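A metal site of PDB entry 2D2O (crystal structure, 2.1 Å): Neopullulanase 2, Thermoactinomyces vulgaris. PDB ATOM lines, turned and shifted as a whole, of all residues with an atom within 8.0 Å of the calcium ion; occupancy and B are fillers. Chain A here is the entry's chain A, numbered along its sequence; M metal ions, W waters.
The side-chain carboxylate (OD1) of Asp 171 is in hydrogen-bond range of the backbone NH (N) of Gly 144, 2.9 Å away. The backbone NH (N) of Asp 171 sits at hydrogen-bond distance from the backbone carbonyl oxygen (O) of Ala 142. OD1 of Asp 171 sits at hydrogen-bond distance from N of Lys 173 (3.2 Å). The side-chain carboxylate (OD1) of Asp 171 lies within hydrogen-bond range of the backbone NH (N) of Gly 174 (2.7 Å). The backbone NH (N) of Asp 171 lies within hydrogen-bond range of the backbone carbonyl oxygen (O) of Pro 138 (3.4 Å). The side-chain carboxylate of Asp 145 lies within hydrogen-bond range of the side-chain hydroxyl of Ser 147, 2.6 Å away. The side-chain amide nitrogen of Asn 148 sits close to the backbone carbonyl oxygen of Gln 215, 3.2 Å away. N of Gly 169 lies within hydrogen-bond range of OE1 of Glu 139 (2.8 Å).
Along chain A the residues within 4 Å of the calcium ion span positions 143 to 171. The nearest printed residue that does not touch the calcium ion is Pro 146 (4.1 Å).
The calcium ion is bound by OD2 of Asp 149 (2.2 Å), water W1 (2.3 Å), OD2 of Asp 171 (2.3 Å), O of Asp 145 (2.4 Å), OD1 of Asn 148 (2.4 Å), O of Gly 169 (2.5 Å) and OD1 of Asn 143 (2.5 Å).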
ATOM      1  N   PRO A 138      -3.955  15.782  15.709  1.00  0.00           N
ATOM      2  CA  PRO A 138      -2.740  15.346  16.407  1.00  0.00           C
ATOM      3  C   PRO A 138      -2.739  15.094  17.916  1.00  0.00           C
ATOM      4  O   PRO A 138      -2.153  14.116  18.365  1.00  0.00           O
ATOM      5  CB  PRO A 138      -1.694  16.368  15.960  1.00  0.00           C
ATOM      6  CG  PRO A 138      -2.498  17.569  15.583  1.00  0.00           C
ATOM      7  CD  PRO A 138      -3.672  16.972  14.883  1.00  0.00           C
ATOM      8  N   GLU A 139      -3.386  15.949  18.701  1.00  0.00           N
ATOM      9  CA  GLU A 139      -3.398  15.749  20.144  1.00  0.00           C
ATOM     10  C   GLU A 139      -4.118  14.456  20.530  1.00  0.00           C
ATOM     11  O   GLU A 139      -3.925  13.954  21.635  1.00  0.00           O
ATOM     12  CB  GLU A 139      -4.059  16.934  20.861  1.00  0.00           C
ATOM     13  CG  GLU A 139      -3.349  17.395  22.154  1.00  0.00           C
ATOM     14  CD  GLU A 139      -3.469  16.414  23.329  1.00  0.00           C
ATOM     15  OE1 GLU A 139      -2.424  16.117  23.960  1.00  0.00           O
ATOM     16  OE2 GLU A 139      -4.593  15.952  23.618  1.00  0.00           O
ATOM     17  N   ALA A 142      -2.148   9.719  18.043  1.00  0.00           N
ATOM     18  CA  ALA A 142      -1.218   8.741  18.575  1.00  0.00           C
ATOM     19  C   ALA A 142      -0.102   9.376  19.395  1.00  0.00           C
ATOM     20  O   ALA A 142       0.550  10.322  18.963  1.00  0.00           O
ATOM     21  CB  ALA A 142      -0.626   7.920  17.437  1.00  0.00           C
ATOM     22  N   ASN A 143       0.100   8.845  20.602  1.00  0.00           N
ATOM     23  CA  ASN A 143       1.124   9.350  21.498  1.00  0.00           C
ATOM     24  C   ASN A 143       2.390   8.512  21.290  1.00  0.00           C
ATOM     25  O   ASN A 143       2.583   7.505  21.971  1.00  0.00           O
ATOM     26  CB  ASN A 143       0.680   9.248  22.958  1.00  0.00           C
ATOM     27  CG  ASN A 143       1.649   9.957  23.895  1.00  0.00           C
ATOM     28  OD1 ASN A 143       2.775  10.272  23.521  1.00  0.00           O
ATOM     29  ND2 ASN A 143       1.202  10.198  25.133  1.00  0.00           N
ATOM     30  N   GLY A 144       3.231   8.927  20.361  1.00  0.00           N
ATOM     31  CA  GLY A 144       4.448   8.182  20.088  1.00  0.00           C
ATOM     32  C   GLY A 144       5.591   8.554  21.016  1.00  0.00           C
ATOM     33  O   GLY A 144       6.541   7.793  21.179  1.00  0.00           O
ATOM     34  N   ASP A 145       5.491   9.724  21.633  1.00  0.00           N
ATOM     35  CA  ASP A 145       6.532  10.202  22.551  1.00  0.00           C
ATOM     36  C   ASP A 145       5.912  10.662  23.854  1.00  0.00           C
ATOM     37  O   ASP A 145       5.481  11.808  23.957  1.00  0.00           O
ATOM     38  CB  ASP A 145       7.297  11.350  21.905  1.00  0.00           C
ATOM     39  CG  ASP A 145       8.385  11.924  22.815  1.00  0.00           C
ATOM     40  OD1 ASP A 145       8.597  11.403  23.935  1.00  0.00           O
ATOM     41  OD2 ASP A 145       9.052  12.893  22.395  1.00  0.00           O
ATOM     42  N   PRO A 146       5.862   9.790  24.871  1.00  0.00           N
ATOM     43  CA  PRO A 146       5.276  10.166  26.160  1.00  0.00           C
ATOM     44  C   PRO A 146       6.047  11.236  26.938  1.00  0.00           C
ATOM     45  O   PRO A 146       5.488  11.835  27.868  1.00  0.00           O
ATOM     46  CB  PRO A 146       5.215   8.839  26.913  1.00  0.00           C
ATOM     47  CG  PRO A 146       6.400   8.100  26.378  1.00  0.00           C
ATOM     48  CD  PRO A 146       6.314   8.382  24.890  1.00  0.00           C
ATOM     49  N   SER A 147       7.296  11.489  26.565  1.00  0.00           N
ATOM     50  CA  SER A 147       8.091  12.486  27.294  1.00  0.00           C
ATOM     51  C   SER A 147       7.722  13.935  27.011  1.00  0.00           C
ATOM     52  O   SER A 147       8.044  14.824  27.801  1.00  0.00           O
ATOM     53  CB  SER A 147       9.599  12.266  27.031  1.00  0.00           C
ATOM     54  OG  SER A 147       9.978  12.634  25.713  1.00  0.00           O
ATOM     55  N   ASN A 148       7.037  14.196  25.904  1.00  0.00           N
ATOM     56  CA  ASN A 148       6.641  15.570  25.567  1.00  0.00           C
ATOM     57  C   ASN A 148       5.174  15.853  25.904  1.00  0.00           C
ATOM     58  O   ASN A 148       4.628  16.886  25.506  1.00  0.00           O
ATOM     59  CB  ASN A 148       6.886  15.861  24.080  1.00  0.00           C
ATOM     60  CG  ASN A 148       6.007  15.004  23.166  1.00  0.00           C
ATOM     61  OD1 ASN A 148       4.990  14.472  23.587  1.00  0.00           O
ATOM     62  ND2 ASN A 148       6.411  14.879  21.901  1.00  0.00           N
ATOM     63  N   ASP A 149       4.531  14.937  26.626  1.00  0.00           N
ATOM     64  CA  ASP A 149       3.123  15.091  26.981  1.00  0.00           C
ATOM     65  C   ASP A 149       2.833  16.315  27.813  1.00  0.00           C
ATOM     66  O   ASP A 149       3.605  16.681  28.701  1.00  0.00           O
ATOM     67  CB  ASP A 149       2.615  13.860  27.732  1.00  0.00           C
ATOM     68  CG  ASP A 149       2.508  12.648  26.842  1.00  0.00           C
ATOM     69  OD1 ASP A 149       2.076  11.593  27.345  1.00  0.00           O
ATOM     70  OD2 ASP A 149       2.855  12.757  25.647  1.00  0.00           O
ATOM     71  N   PRO A 150       1.693  16.973  27.551  1.00  0.00           N
ATOM     72  CA  PRO A 150       1.298  18.177  28.292  1.00  0.00           C
ATOM     73  C   PRO A 150       1.028  17.818  29.749  1.00  0.00           C
ATOM     74  O   PRO A 150       1.039  16.640  30.125  1.00  0.00           O
ATOM     75  CB  PRO A 150       0.013  18.609  27.583  1.00  0.00           C
ATOM     76  CG  PRO A 150       0.159  18.040  26.196  1.00  0.00           C
ATOM     77  CD  PRO A 150       0.738  16.683  26.472  1.00  0.00           C
ATOM     78  N   THR A 153      -2.031  15.163  31.529  1.00  0.00           N
ATOM     79  CA  THR A 153      -2.459  14.314  30.435  1.00  0.00           C
ATOM     80  C   THR A 153      -3.316  13.199  31.030  1.00  0.00           C
ATOM     81  O   THR A 153      -2.949  12.605  32.036  1.00  0.00           O
ATOM     82  CB  THR A 153      -1.254  13.699  29.700  1.00  0.00           C
ATOM     83  OG1 THR A 153      -0.610  14.718  28.923  1.00  0.00           O
ATOM     84  CG2 THR A 153      -1.698  12.574  28.774  1.00  0.00           C
ATOM     85  N   TRP A 156      -5.296   7.323  28.018  1.00  0.00           N
ATOM     86  CA  TRP A 156      -5.659   7.052  26.637  1.00  0.00           C
ATOM     87  C   TRP A 156      -6.552   5.817  26.634  1.00  0.00           C
ATOM     88  O   TRP A 156      -6.053   4.694  26.488  1.00  0.00           O
ATOM     89  CB  TRP A 156      -4.401   6.799  25.814  1.00  0.00           C
ATOM     90  CG  TRP A 156      -4.613   6.895  24.337  1.00  0.00           C
ATOM     91  CD1 TRP A 156      -5.285   6.009  23.537  1.00  0.00           C
ATOM     92  CD2 TRP A 156      -4.163   7.938  23.471  1.00  0.00           C
ATOM     93  NE1 TRP A 156      -5.258   6.430  22.230  1.00  0.00           N
ATOM     94  CE2 TRP A 156      -4.581   7.611  22.163  1.00  0.00           C
ATOM     95  CE3 TRP A 156      -3.426   9.116  23.675  1.00  0.00           C
ATOM     96  CZ2 TRP A 156      -4.301   8.430  21.059  1.00  0.00           C
ATOM     97  CZ3 TRP A 156      -3.146   9.935  22.572  1.00  0.00           C
ATOM     98  CH2 TRP A 156      -3.588   9.585  21.277  1.00  0.00           C
ATOM     99  N   TYR A 168      -4.250  14.343  25.979  1.00  0.00           N
ATOM    100  CA  TYR A 168      -4.019  12.898  25.999  1.00  0.00           C
ATOM    101  C   TYR A 168      -2.604  12.540  25.532  1.00  0.00           C
ATOM    102  O   TYR A 168      -2.199  11.388  25.616  1.00  0.00           O
ATOM    103  CB  TYR A 168      -5.066  12.181  25.131  1.00  0.00           C
ATOM    104  CG  TYR A 168      -6.452  12.250  25.738  1.00  0.00           C
ATOM    105  CD1 TYR A 168      -6.894  11.259  26.627  1.00  0.00           C
ATOM    106  CD2 TYR A 168      -7.296  13.326  25.470  1.00  0.00           C
ATOM    107  CE1 TYR A 168      -8.155  11.351  27.235  1.00  0.00           C
ATOM    108  CE2 TYR A 168      -8.545  13.426  26.074  1.00  0.00           C
ATOM    109  CZ  TYR A 168      -8.971  12.442  26.946  1.00  0.00           C
ATOM    110  OH  TYR A 168     -10.221  12.534  27.528  1.00  0.00           O
ATOM    111  N   GLY A 169      -1.874  13.530  25.021  1.00  0.00           N
ATOM    112  CA  GLY A 169      -0.498  13.300  24.596  1.00  0.00           C
ATOM    113  C   GLY A 169      -0.220  12.964  23.147  1.00  0.00           C
ATOM    114  O   GLY A 169       0.917  12.622  22.817  1.00  0.00           O
ATOM    115  N   GLY A 170      -1.220  13.065  22.266  1.00  0.00           N
ATOM    116  CA  GLY A 170      -0.985  12.751  20.868  1.00  0.00           C
ATOM    117  C   GLY A 170       0.111  13.628  20.293  1.00  0.00           C
ATOM    118  O   GLY A 170       0.223  14.799  20.657  1.00  0.00           O
ATOM    119  N   ASP A 171       0.939  13.078  19.401  1.00  0.00           N
ATOM    120  CA  ASP A 171       2.025  13.862  18.818  1.00  0.00           C
ATOM    121  C   ASP A 171       2.426  13.417  17.409  1.00  0.00           C
ATOM    122  O   ASP A 171       1.891  12.448  16.867  1.00  0.00           O
ATOM    123  CB  ASP A 171       3.256  13.800  19.730  1.00  0.00           C
ATOM    124  CG  ASP A 171       3.641  12.385  20.109  1.00  0.00           C
ATOM    125  OD1 ASP A 171       3.740  11.540  19.180  1.00  0.00           O
ATOM    126  OD2 ASP A 171       3.861  12.125  21.315  1.00  0.00           O
ATOM    127  N   LEU A 172       3.399  14.122  16.831  1.00  0.00           N
ATOM    128  CA  LEU A 172       3.872  13.820  15.483  1.00  0.00           C
ATOM    129  C   LEU A 172       4.627  12.498  15.386  1.00  0.00           C
ATOM    130  O   LEU A 172       4.590  11.829  14.349  1.00  0.00           O
ATOM    131  CB  LEU A 172       4.755  14.954  14.958  1.00  0.00           C
ATOM    132  CG  LEU A 172       4.082  16.319  14.820  1.00  0.00           C
ATOM    133  CD1 LEU A 172       5.062  17.298  14.185  1.00  0.00           C
ATOM    134  CD2 LEU A 172       2.824  16.191  13.971  1.00  0.00           C
ATOM    135  N   LYS A 173       5.333  12.137  16.458  1.00  0.00           N
ATOM    136  CA  LYS A 173       6.071  10.883  16.451  1.00  0.00           C
ATOM    137  C   LYS A 173       5.060   9.746  16.310  1.00  0.00           C
ATOM    138  O   LYS A 173       5.286   8.772  15.591  1.00  0.00           O
ATOM    139  CB  LYS A 173       6.894  10.734  17.735  1.00  0.00           C
ATOM    140  CG  LYS A 173       7.619   9.394  17.868  1.00  0.00           C
ATOM    141  CD  LYS A 173       8.448   9.074  16.631  1.00  0.00           C
ATOM    142  CE  LYS A 173       9.222   7.767  16.796  1.00  0.00           C
ATOM    143  NZ  LYS A 173      10.093   7.796  18.025  1.00  0.00           N
ATOM    144  N   GLY A 174       3.926   9.873  17.001  1.00  0.00           N
ATOM    145  CA  GLY A 174       2.891   8.866  16.923  1.00  0.00           C
ATOM    146  C   GLY A 174       2.400   8.703  15.485  1.00  0.00           C
ATOM    147  O   GLY A 174       2.255   7.587  14.994  1.00  0.00           O
ATOM    148  N   PRO A 214       5.941  22.159  21.004  1.00  0.00           N
ATOM    149  CA  PRO A 214       6.773  21.223  21.762  1.00  0.00           C
ATOM    150  C   PRO A 214       6.066  19.908  22.146  1.00  0.00           C
ATOM    151  O   PRO A 214       6.704  18.848  22.187  1.00  0.00           O
ATOM    152  CB  PRO A 214       7.190  22.042  22.981  1.00  0.00           C
ATOM    153  CG  PRO A 214       7.267  23.438  22.428  1.00  0.00           C
ATOM    154  CD  PRO A 214       5.990  23.509  21.611  1.00  0.00           C
ATOM    155  N   GLN A 215       4.760  19.980  22.421  1.00  0.00           N
ATOM    156  CA  GLN A 215       3.999  18.795  22.774  1.00  0.00           C
ATOM    157  C   GLN A 215       3.907  17.857  21.573  1.00  0.00           C
ATOM    158  O   GLN A 215       3.724  16.653  21.727  1.00  0.00           O
ATOM    159  CB  GLN A 215       2.577  19.157  23.201  1.00  0.00           C
ATOM    160  CG  GLN A 215       2.472  20.183  24.334  1.00  0.00           C
ATOM    161  CD  GLN A 215       1.034  20.654  24.548  1.00  0.00           C
ATOM    162  OE1 GLN A 215       0.148  20.377  23.742  1.00  0.00           O
ATOM    163  NE2 GLN A 215       0.809  21.386  25.644  1.00  0.00           N
ATOM    164  N   PHE A 216       4.010  18.424  20.373  1.00  0.00           N
ATOM    165  CA  PHE A 216       3.904  17.626  19.148  1.00  0.00           C
ATOM    166  C   PHE A 216       5.260  17.210  18.593  1.00  0.00           C
ATOM    167  O   PHE A 216       5.345  16.225  17.852  1.00  0.00           O
ATOM    168  CB  PHE A 216       3.131  18.394  18.070  1.00  0.00           C
ATOM    169  CG  PHE A 216       1.659  18.561  18.363  1.00  0.00           C
ATOM    170  CD1 PHE A 216       1.006  17.741  19.289  1.00  0.00           C
ATOM    171  CD2 PHE A 216       0.911  19.506  17.666  1.00  0.00           C
ATOM    172  CE1 PHE A 216      -0.365  17.862  19.523  1.00  0.00           C
ATOM    173  CE2 PHE A 216      -0.467  19.633  17.889  1.00  0.00           C
ATOM    174  CZ  PHE A 216      -1.110  18.801  18.820  1.00  0.00           C
ATOM    175  N   GLY A 217       6.311  17.949  18.926  1.00  0.00           N
ATOM    176  CA  GLY A 217       7.628  17.603  18.429  1.00  0.00           C
ATOM    177  C   GLY A 217       8.476  18.825  18.122  1.00  0.00           C
ATOM    178  O   GLY A 217       8.351  19.846  18.787  1.00  0.00           O
HETATM  179 CA    CA M   1       3.298  12.713  23.474  1.00  0.00          CA
HETATM  180  O   HOH W   1       2.451  14.842  23.651  1.00  0.00           O
